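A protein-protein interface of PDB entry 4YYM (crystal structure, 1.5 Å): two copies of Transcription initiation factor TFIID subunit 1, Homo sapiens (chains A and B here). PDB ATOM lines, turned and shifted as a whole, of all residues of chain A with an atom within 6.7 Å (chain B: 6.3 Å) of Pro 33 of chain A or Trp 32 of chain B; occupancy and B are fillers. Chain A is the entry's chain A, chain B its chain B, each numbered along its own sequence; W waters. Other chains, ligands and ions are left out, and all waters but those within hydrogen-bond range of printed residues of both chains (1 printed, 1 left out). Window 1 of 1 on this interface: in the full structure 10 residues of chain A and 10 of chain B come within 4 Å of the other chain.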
ATOM      1  N   ASP A  30       1.243  -9.499 -18.268  1.00  0.00           N
ATOM      2  CA  ASP A  30       1.477 -10.771 -17.557  1.00  0.00           C
ATOM      3  C   ASP A  30       0.861 -11.944 -18.347  1.00  0.00           C
ATOM      4  O   ASP A  30       0.354 -12.927 -17.781  1.00  0.00           O
ATOM      5  CB  ASP A  30       0.964 -10.652 -16.101  1.00  0.00           C
ATOM      6  CG  ASP A  30       1.449  -9.360 -15.434  1.00  0.00           C
ATOM      7  OD1 ASP A  30       2.643  -8.986 -15.604  1.00  0.00           O
ATOM      8  OD2 ASP A  30       0.620  -8.663 -14.814  1.00  0.00           O
ATOM      9  N   SER A  31       0.904 -11.813 -19.679  1.00  0.00           N
ATOM     10  CA  SER A  31       0.260 -12.792 -20.579  1.00  0.00           C
ATOM     11  C   SER A  31       1.190 -13.797 -21.091  1.00  0.00           C
ATOM     12  O   SER A  31       0.738 -14.575 -21.942  1.00  0.00           O
ATOM     13  CB  SER A  31      -0.406 -12.108 -21.719  1.00  0.00           C
ATOM     14  OG  SER A  31       0.501 -11.410 -22.575  1.00  0.00           O
ATOM     15  N   TRP A  32       2.383 -13.918 -20.483  1.00  0.00           N
ATOM     16  CA  TRP A  32       3.463 -14.855 -20.919  1.00  0.00           C
ATOM     17  C   TRP A  32       3.006 -16.306 -21.242  1.00  0.00           C
ATOM     18  O   TRP A  32       3.452 -16.869 -22.201  1.00  0.00           O
ATOM     19  CB  TRP A  32       4.564 -14.890 -19.822  1.00  0.00           C
ATOM     20  CG  TRP A  32       4.993 -13.521 -19.438  1.00  0.00           C
ATOM     21  CD1 TRP A  32       4.858 -12.925 -18.206  1.00  0.00           C
ATOM     22  CD2 TRP A  32       5.603 -12.563 -20.318  1.00  0.00           C
ATOM     23  NE1 TRP A  32       5.341 -11.617 -18.292  1.00  0.00           N
ATOM     24  CE2 TRP A  32       5.820 -11.378 -19.549  1.00  0.00           C
ATOM     25  CE3 TRP A  32       6.037 -12.590 -21.661  1.00  0.00           C
ATOM     26  CZ2 TRP A  32       6.431 -10.237 -20.076  1.00  0.00           C
ATOM     27  CZ3 TRP A  32       6.651 -11.418 -22.203  1.00  0.00           C
ATOM     28  CH2 TRP A  32       6.825 -10.262 -21.417  1.00  0.00           C
ATOM     29  N   PRO A  33       2.138 -16.891 -20.408  1.00  0.00           N
ATOM     30  CA  PRO A  33       1.757 -18.280 -20.630  1.00  0.00           C
ATOM     31  C   PRO A  33       1.069 -18.489 -21.957  1.00  0.00           C
ATOM     32  O   PRO A  33       1.221 -19.564 -22.586  1.00  0.00           O
ATOM     33  CB  PRO A  33       0.723 -18.517 -19.504  1.00  0.00           C
ATOM     34  CG  PRO A  33       1.167 -17.617 -18.398  1.00  0.00           C
ATOM     35  CD  PRO A  33       1.554 -16.368 -19.154  1.00  0.00           C
ATOM     36  N   PHE A  34       0.459 -17.440 -22.528  1.00  0.00           N
ATOM     37  CA  PHE A  34      -0.124 -17.549 -23.797  1.00  0.00           C
ATOM     38  C   PHE A  34       0.831 -17.358 -24.990  1.00  0.00           C
ATOM     39  O   PHE A  34       0.417 -17.435 -26.145  1.00  0.00           O
ATOM     40  CB  PHE A  34      -1.279 -16.516 -23.910  1.00  0.00           C
ATOM     41  CG  PHE A  34      -2.399 -16.815 -23.016  1.00  0.00           C
ATOM     42  CD1 PHE A  34      -3.304 -17.856 -23.370  1.00  0.00           C
ATOM     43  CD2 PHE A  34      -2.534 -16.218 -21.741  1.00  0.00           C
ATOM     44  CE1 PHE A  34      -4.379 -18.153 -22.539  1.00  0.00           C
ATOM     45  CE2 PHE A  34      -3.618 -16.556 -20.959  1.00  0.00           C
ATOM     46  CZ  PHE A  34      -4.501 -17.550 -21.292  1.00  0.00           C
ATOM     47  N   HIS A  35       2.091 -17.052 -24.674  1.00  0.00           N
ATOM     48  CA  HIS A  35       3.063 -16.792 -25.735  1.00  0.00           C
ATOM     49  C   HIS A  35       3.790 -18.082 -26.172  1.00  0.00           C
ATOM     50  O   HIS A  35       4.616 -17.962 -27.052  1.00  0.00           O
ATOM     51  CB  HIS A  35       4.201 -15.872 -25.265  1.00  0.00           C
ATOM     52  CG  HIS A  35       3.745 -14.494 -24.823  1.00  0.00           C
ATOM     53  ND1 HIS A  35       4.606 -13.396 -24.785  1.00  0.00           N
ATOM     54  CD2 HIS A  35       2.512 -14.034 -24.446  1.00  0.00           C
ATOM     55  CE1 HIS A  35       3.904 -12.332 -24.397  1.00  0.00           C
ATOM     56  NE2 HIS A  35       2.664 -12.703 -24.128  1.00  0.00           N
ATOM     57  N   HIS A  36       3.525 -19.270 -25.589  1.00  0.00           N
ATOM     58  CA  HIS A  36       4.275 -20.482 -25.937  1.00  0.00           C
ATOM     59  C   HIS A  36       3.273 -21.598 -25.918  1.00  0.00           C
ATOM     60  O   HIS A  36       2.287 -21.601 -25.144  1.00  0.00           O
ATOM     61  CB  HIS A  36       5.216 -20.832 -24.799  1.00  0.00           C
ATOM     62  CG  HIS A  36       6.123 -19.705 -24.474  1.00  0.00           C
ATOM     63  ND1 HIS A  36       7.251 -19.469 -25.203  1.00  0.00           N
ATOM     64  CD2 HIS A  36       6.076 -18.735 -23.508  1.00  0.00           C
ATOM     65  CE1 HIS A  36       7.879 -18.412 -24.710  1.00  0.00           C
ATOM     66  NE2 HIS A  36       7.160 -17.925 -23.712  1.00  0.00           N
ATOM     67  N   PRO A  37       3.533 -22.649 -26.711  1.00  0.00           N
ATOM     68  CA  PRO A  37       2.674 -23.834 -26.645  1.00  0.00           C
ATOM     69  C   PRO A  37       2.727 -24.484 -25.270  1.00  0.00           C
ATOM     70  O   PRO A  37       3.716 -24.325 -24.553  1.00  0.00           O
ATOM     71  CB  PRO A  37       3.258 -24.765 -27.705  1.00  0.00           C
ATOM     72  CG  PRO A  37       4.286 -24.004 -28.428  1.00  0.00           C
ATOM     73  CD  PRO A  37       4.559 -22.700 -27.760  1.00  0.00           C
ATOM     74  N   VAL A  38       1.627 -25.118 -24.853  1.00  0.00           N
ATOM     75  CA  VAL A  38       1.718 -25.954 -23.650  1.00  0.00           C
ATOM     76  C   VAL A  38       2.525 -27.246 -23.881  1.00  0.00           C
ATOM     77  O   VAL A  38       2.324 -28.022 -24.838  1.00  0.00           O
ATOM     78  CB  VAL A  38       0.300 -26.310 -23.171  1.00  0.00           C
ATOM     79  CG1 VAL A  38       0.365 -27.097 -21.883  1.00  0.00           C
ATOM     80  CG2 VAL A  38      -0.517 -25.102 -22.889  1.00  0.00           C
ATOM     81  N   ASN A  39       3.507 -27.453 -22.979  1.00  0.00           N
ATOM     82  CA  ASN A  39       4.321 -28.678 -22.950  1.00  0.00           C
ATOM     83  C   ASN A  39       3.743 -29.654 -21.898  1.00  0.00           C
ATOM     84  O   ASN A  39       3.543 -29.255 -20.740  1.00  0.00           O
ATOM     85  CB  ASN A  39       5.760 -28.294 -22.626  1.00  0.00           C
ATOM     86  CG  ASN A  39       6.759 -29.425 -22.912  1.00  0.00           C
ATOM     87  OD1 ASN A  39       6.431 -30.640 -22.849  1.00  0.00           O
ATOM     88  ND2 ASN A  39       8.028 -29.031 -23.221  1.00  0.00           N
ATOM     89  N   PHE A  42       4.923 -30.123 -18.106  1.00  0.00           N
ATOM     90  CA  PHE A  42       4.476 -29.223 -17.067  1.00  0.00           C
ATOM     91  C   PHE A  42       3.016 -29.168 -16.783  1.00  0.00           C
ATOM     92  O   PHE A  42       2.632 -28.794 -15.723  1.00  0.00           O
ATOM     93  CB  PHE A  42       4.864 -27.752 -17.438  1.00  0.00           C
ATOM     94  CG  PHE A  42       6.331 -27.403 -17.315  1.00  0.00           C
ATOM     95  CD1 PHE A  42       7.205 -28.087 -16.470  1.00  0.00           C
ATOM     96  CD2 PHE A  42       6.848 -26.287 -18.027  1.00  0.00           C
ATOM     97  CE1 PHE A  42       8.523 -27.735 -16.384  1.00  0.00           C
ATOM     98  CE2 PHE A  42       8.209 -25.924 -17.935  1.00  0.00           C
ATOM     99  CZ  PHE A  42       9.027 -26.642 -17.098  1.00  0.00           C
ATOM    100  N   ASP A  55      -1.214 -20.861 -29.596  1.00  0.00           N
ATOM    101  CA  ASP A  55      -0.489 -19.868 -28.736  1.00  0.00           C
ATOM    102  C   ASP A  55       0.029 -18.767 -29.681  1.00  0.00           C
ATOM    103  O   ASP A  55       0.063 -18.941 -30.891  1.00  0.00           O
ATOM    104  CB  ASP A  55       0.611 -20.523 -27.954  1.00  0.00           C
ATOM    105  CG  ASP A  55       1.695 -21.064 -28.877  1.00  0.00           C
ATOM    106  OD1 ASP A  55       1.551 -22.227 -29.452  1.00  0.00           O
ATOM    107  OD2 ASP A  55       2.631 -20.294 -29.243  1.00  0.00           O
ATOM    108  N   TYR A  95      -7.004 -17.021 -16.069  1.00  0.00           N
ATOM    109  CA  TYR A  95      -6.333 -17.313 -17.372  1.00  0.00           C
ATOM    110  C   TYR A  95      -7.270 -16.934 -18.507  1.00  0.00           C
ATOM    111  O   TYR A  95      -6.852 -16.286 -19.457  1.00  0.00           O
ATOM    112  CB  TYR A  95      -6.003 -18.813 -17.499  1.00  0.00           C
ATOM    113  CG  TYR A  95      -4.857 -19.281 -16.665  1.00  0.00           C
ATOM    114  CD1 TYR A  95      -3.546 -18.994 -17.046  1.00  0.00           C
ATOM    115  CD2 TYR A  95      -5.084 -20.062 -15.521  1.00  0.00           C
ATOM    116  CE1 TYR A  95      -2.448 -19.422 -16.259  1.00  0.00           C
ATOM    117  CE2 TYR A  95      -4.027 -20.492 -14.760  1.00  0.00           C
ATOM    118  CZ  TYR A  95      -2.721 -20.150 -15.121  1.00  0.00           C
ATOM    119  OH  TYR A  95      -1.725 -20.666 -14.295  1.00  0.00           O
ATOM    120  N   THR A  98      -7.486 -13.239 -19.078  1.00  0.00           N
ATOM    121  CA  THR A  98      -6.384 -12.724 -19.870  1.00  0.00           C
ATOM    122  C   THR A  98      -6.526 -13.101 -21.348  1.00  0.00           C
ATOM    123  O   THR A  98      -6.248 -12.274 -22.243  1.00  0.00           O
ATOM    124  CB  THR A  98      -5.082 -13.228 -19.273  1.00  0.00           C
ATOM    125  OG1 THR A  98      -4.911 -12.723 -17.957  1.00  0.00           O
ATOM    126  CG2 THR A  98      -3.863 -12.863 -20.122  1.00  0.00           C
ATOM    127  N   MET B  26      18.642 -18.230 -19.900  1.00  0.00           N
ATOM    128  CA  MET B  26      17.397 -18.096 -20.631  1.00  0.00           C
ATOM    129  C   MET B  26      17.305 -19.055 -21.830  1.00  0.00           C
ATOM    130  O   MET B  26      16.174 -19.251 -22.312  1.00  0.00           O
ATOM    131  CB  MET B  26      17.189 -16.695 -21.134  1.00  0.00           C
ATOM    132  CG  MET B  26      16.854 -15.793 -19.919  1.00  0.00           C
ATOM    133  SD  MET B  26      16.637 -14.047 -20.383  1.00  0.00           S
ATOM    134  CE  MET B  26      15.141 -13.989 -21.393  1.00  0.00           C
ATOM    135  N   VAL B  28      18.075 -22.220 -21.642  1.00  0.00           N
ATOM    136  CA  VAL B  28      17.784 -23.594 -21.151  1.00  0.00           C
ATOM    137  C   VAL B  28      16.420 -24.011 -21.760  1.00  0.00           C
ATOM    138  O   VAL B  28      15.482 -23.243 -21.752  1.00  0.00           O
ATOM    139  CB  VAL B  28      17.773 -23.663 -19.606  1.00  0.00           C
ATOM    140  CG1 VAL B  28      17.151 -24.968 -19.120  1.00  0.00           C
ATOM    141  CG2 VAL B  28      19.175 -23.466 -19.002  1.00  0.00           C
ATOM    142  N   PRO B  29      16.294 -25.246 -22.321  1.00  0.00           N
ATOM    143  CA  PRO B  29      14.968 -25.477 -22.907  1.00  0.00           C
ATOM    144  C   PRO B  29      13.813 -25.474 -21.910  1.00  0.00           C
ATOM    145  O   PRO B  29      13.975 -25.935 -20.764  1.00  0.00           O
ATOM    146  CB  PRO B  29      15.090 -26.887 -23.522  1.00  0.00           C
ATOM    147  CG  PRO B  29      16.545 -27.187 -23.593  1.00  0.00           C
ATOM    148  CD  PRO B  29      17.243 -26.362 -22.511  1.00  0.00           C
ATOM    149  N   ASP B  30      12.685 -24.922 -22.367  1.00  0.00           N
ATOM    150  CA  ASP B  30      11.481 -24.850 -21.531  1.00  0.00           C
ATOM    151  C   ASP B  30      11.679 -24.060 -20.268  1.00  0.00           C
ATOM    152  O   ASP B  30      10.942 -24.181 -19.260  1.00  0.00           O
ATOM    153  CB  ASP B  30      10.969 -26.235 -21.158  1.00  0.00           C
ATOM    154  CG  ASP B  30      10.719 -27.065 -22.383  1.00  0.00           C
ATOM    155  OD1 ASP B  30       9.856 -26.647 -23.177  1.00  0.00           O
ATOM    156  OD2 ASP B  30      11.405 -28.080 -22.585  1.00  0.00           O
ATOM    157  N   SER B  31      12.586 -23.117 -20.385  1.00  0.00           N
ATOM    158  CA  SER B  31      12.912 -22.334 -19.175  1.00  0.00           C
ATOM    159  C   SER B  31      11.970 -21.104 -19.080  1.00  0.00           C
ATOM    160  O   SER B  31      11.935 -20.423 -18.044  1.00  0.00           O
ATOM    161  CB  SER B  31      14.365 -21.749 -19.155  1.00  0.00           C
ATOM    162  OG  SER B  31      14.673 -20.995 -20.293  1.00  0.00           O
ATOM    163  N   TRP B  32      11.248 -20.831 -20.148  1.00  0.00           N
ATOM    164  CA  TRP B  32      10.362 -19.624 -20.115  1.00  0.00           C
ATOM    165  C   TRP B  32       9.499 -19.327 -18.861  1.00  0.00           C
ATOM    166  O   TRP B  32       9.405 -18.137 -18.531  1.00  0.00           O
ATOM    167  CB  TRP B  32       9.643 -19.385 -21.451  1.00  0.00           C
ATOM    168  CG  TRP B  32       8.585 -20.333 -21.555  1.00  0.00           C
ATOM    169  CD1 TRP B  32       8.624 -21.516 -22.253  1.00  0.00           C
ATOM    170  CD2 TRP B  32       7.272 -20.213 -20.993  1.00  0.00           C
ATOM    171  NE1 TRP B  32       7.416 -22.181 -22.095  1.00  0.00           N
ATOM    172  CE2 TRP B  32       6.557 -21.417 -21.348  1.00  0.00           C
ATOM    173  CE3 TRP B  32       6.644 -19.247 -20.179  1.00  0.00           C
ATOM    174  CZ2 TRP B  32       5.240 -21.676 -20.912  1.00  0.00           C
ATOM    175  CZ3 TRP B  32       5.329 -19.478 -19.722  1.00  0.00           C
ATOM    176  CH2 TRP B  32       4.615 -20.690 -20.143  1.00  0.00           C
ATOM    177  N   PRO B  33       9.002 -20.308 -18.080  1.00  0.00           N
ATOM    178  CA  PRO B  33       8.173 -19.962 -16.910  1.00  0.00           C
ATOM    179  C   PRO B  33       9.015 -19.273 -15.885  1.00  0.00           C
ATOM    180  O   PRO B  33       8.455 -18.636 -15.014  1.00  0.00           O
ATOM    181  CB  PRO B  33       7.733 -21.306 -16.398  1.00  0.00           C
ATOM    182  CG  PRO B  33       7.637 -22.146 -17.695  1.00  0.00           C
ATOM    183  CD  PRO B  33       8.854 -21.760 -18.418  1.00  0.00           C
ATOM    184  N   PHE B  34      10.328 -19.433 -15.995  1.00  0.00           N
ATOM    185  CA  PHE B  34      11.302 -18.741 -15.096  1.00  0.00           C
ATOM    186  C   PHE B  34      11.750 -17.411 -15.574  1.00  0.00           C
ATOM    187  O   PHE B  34      12.529 -16.732 -14.845  1.00  0.00           O
ATOM    188  CB  PHE B  34      12.489 -19.621 -14.843  1.00  0.00           C
ATOM    189  CG  PHE B  34      12.096 -20.908 -14.174  1.00  0.00           C
ATOM    190  CD1 PHE B  34      11.985 -20.966 -12.811  1.00  0.00           C
ATOM    191  CD2 PHE B  34      11.912 -22.066 -14.924  1.00  0.00           C
ATOM    192  CE1 PHE B  34      11.627 -22.161 -12.157  1.00  0.00           C
ATOM    193  CE2 PHE B  34      11.497 -23.251 -14.299  1.00  0.00           C
ATOM    194  CZ  PHE B  34      11.398 -23.290 -12.914  1.00  0.00           C
ATOM    195  N   HIS B  35      11.299 -17.009 -16.776  1.00  0.00           N
ATOM    196  CA  HIS B  35      11.781 -15.752 -17.337  1.00  0.00           C
ATOM    197  C   HIS B  35      11.124 -14.482 -16.750  1.00  0.00           C
ATOM    198  O   HIS B  35      11.652 -13.443 -16.966  1.00  0.00           O
ATOM    199  CB  HIS B  35      11.520 -15.767 -18.857  1.00  0.00           C
ATOM    200  CG  HIS B  35      12.423 -16.698 -19.616  1.00  0.00           C
ATOM    201  ND1 HIS B  35      12.660 -16.525 -20.959  1.00  0.00           N
ATOM    202  CD2 HIS B  35      13.101 -17.816 -19.235  1.00  0.00           C
ATOM    203  CE1 HIS B  35      13.462 -17.513 -21.373  1.00  0.00           C
ATOM    204  NE2 HIS B  35      13.739 -18.304 -20.355  1.00  0.00           N
ATOM    205  N   HIS B  36       9.955 -14.601 -16.114  1.00  0.00           N
ATOM    206  CA  HIS B  36       9.223 -13.453 -15.539  1.00  0.00           C
ATOM    207  C   HIS B  36       8.683 -13.875 -14.185  1.00  0.00           C
ATOM    208  O   HIS B  36       8.618 -15.103 -13.911  1.00  0.00           O
ATOM    209  CB  HIS B  36       8.042 -13.181 -16.476  1.00  0.00           C
ATOM    210  CG  HIS B  36       8.480 -12.836 -17.840  1.00  0.00           C
ATOM    211  ND1 HIS B  36       9.108 -11.662 -18.157  1.00  0.00           N
ATOM    212  CD2 HIS B  36       8.515 -13.581 -18.968  1.00  0.00           C
ATOM    213  CE1 HIS B  36       9.410 -11.634 -19.442  1.00  0.00           C
ATOM    214  NE2 HIS B  36       9.083 -12.802 -19.948  1.00  0.00           N
ATOM    215  N   ASN B  39       2.616 -14.695 -12.053  1.00  0.00           N
ATOM    216  CA  ASN B  39       1.418 -13.871 -12.057  1.00  0.00           C
ATOM    217  C   ASN B  39       0.569 -14.231 -10.831  1.00  0.00           C
ATOM    218  O   ASN B  39       0.031 -15.332 -10.755  1.00  0.00           O
ATOM    219  CB  ASN B  39       0.668 -14.135 -13.340  1.00  0.00           C
ATOM    220  CG  ASN B  39      -0.521 -13.186 -13.529  1.00  0.00           C
ATOM    221  OD1 ASN B  39      -1.008 -12.569 -12.559  1.00  0.00           O
ATOM    222  ND2 ASN B  39      -0.951 -13.012 -14.785  1.00  0.00           N
ATOM    223  N   PHE B  42      -2.832 -15.665 -11.567  1.00  0.00           N
ATOM    224  CA  PHE B  42      -2.883 -17.036 -12.073  1.00  0.00           C
ATOM    225  C   PHE B  42      -2.573 -17.942 -10.920  1.00  0.00           C
ATOM    226  O   PHE B  42      -3.184 -19.012 -10.827  1.00  0.00           O
ATOM    227  CB  PHE B  42      -1.883 -17.248 -13.213  1.00  0.00           C
ATOM    228  CG  PHE B  42      -2.167 -16.457 -14.467  1.00  0.00           C
ATOM    229  CD1 PHE B  42      -3.422 -15.864 -14.734  1.00  0.00           C
ATOM    230  CD2 PHE B  42      -1.158 -16.350 -15.465  1.00  0.00           C
ATOM    231  CE1 PHE B  42      -3.655 -15.134 -15.901  1.00  0.00           C
ATOM    232  CE2 PHE B  42      -1.354 -15.642 -16.670  1.00  0.00           C
ATOM    233  CZ  PHE B  42      -2.635 -15.041 -16.914  1.00  0.00           C
ATOM    234  N   THR B  98      13.928 -28.189 -14.411  1.00  0.00           N
ATOM    235  CA  THR B  98      14.248 -27.045 -15.251  1.00  0.00           C
ATOM    236  C   THR B  98      15.030 -26.002 -14.455  1.00  0.00           C
ATOM    237  O   THR B  98      16.075 -25.554 -14.974  1.00  0.00           O
ATOM    238  CB  THR B  98      13.002 -26.494 -15.870  1.00  0.00           C
ATOM    239  OG1 THR B  98      12.425 -27.534 -16.663  1.00  0.00           O
ATOM    240  CG2 THR B  98      13.371 -25.381 -16.824  1.00  0.00           C
HETATM  241  O   HOH W   1      -3.420 -11.316 -15.247  1.00  0.00           O
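The side-chain amide nitrogen of Asn 39 of chain B is in hydrogen-bond range of the backbone carbonyl oxygen of Asp 30 of chain A (3.3 Å). OD1 of Asp 30 of chain B lies within hydrogen-bond range of ND2 of Asn 39 of chain A, at 3.0 Å.
Of the 13 printed residues of chain B, 7 touch a printed residue of chain A. Hydrophobic or aromatic side chains of chain B within 4 Å of the printed part of chain A: Trp 32, Pro 33, His 36 and Phe 42. Hydrophobic or aromatic side chains of chain A within 4 Å of the printed part of chain B: Trp 32, Pro 33, His 36, Phe 42 and Tyr 95. Among the printed residues, no Asp or Glu carboxylate lies within 4 Å of a Lys or Arg side-chain nitrogen of the other chain.
Printed residues of chain B within 4 Å of Phe 42 of chain A: Asp 30 (3.5 Å), Pro 33 (3.8 Å) and Thr 98 (3.5 Å). Of the printed residues of chain B, Tyr 95 of chain A touches Phe 42. Of the printed residues of chain B, Thr 98 of chain A touches Phe 42. Of the printed residues of chain A, Asp 30 of chain B touches Asn 39 (3.0 Å) and Phe 42 (3.5 Å). The nearest residue of chain B that does not touch Pro 33 of chain A is Asn 39 of chain B (6.1 Å). The nearest residue of chain A that does not touch Trp 32 of chain B is Trp 32 of chain A (4.1 Å).
Water W1 bridges ND2 of Asn 39 of chain B (3.0 Å) and OG1 of Thr 98 of chain A (3.4 Å).
Asp 30 of chain A touches Phe 42 of chain B (O to CE2, 3.4 Å). CZ2 of Trp 32 of chain A touches CE1 of His 36 of chain B (3.4 Å). Trp 32 of chain B touches Pro 33 of chain A (CH2 to CA, 3.8 Å). Pro 33 of chain A touches Phe 42 of chain B. CD2 of His 36 of chain A touches CD2 of Trp 32 of chain B, at 3.2 Å. Phe 42 of chain A touches Asp 30 of chain B (CE2 to O, 3.5 Å). Phe 42 of chain A touches Pro 33 of chain B (CE2 to CG, 3.8 Å). OG1 of Thr 98 of chain B touches CZ of Phe 42 of chain A (3.5 Å). CE1 of Tyr 95 of chain A touches CD2 of Phe 42 of chain B (3.4 Å). OG1 of Thr 98 of chain A touches CE1 of Phe 42 of chain B, at 3.4 Å.
Asp 30 of chain A touches Asn 39 of chain B, and with the chains exchanged Asn 39 of chain A touches Asp 30 of chain B. Asp 30 of chain A touches Phe 42 of chain B, and with the chains exchanged Phe 42 of chain A touches Asp 30 of chain B. Trp 32 of chain A touches His 36 of chain B, and with the chains exchanged His 36 of chain A touches Trp 32 of chain B. Pro 33 of chain A touches Trp 32 of chain B, but with the chains exchanged Trp 32 of chain A does not touch Pro 33 of chain B (6.9 Å). Of the 12 pairs that touch across the chains among the printed residues, 10 have their exchanged pair printed and touching as well.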
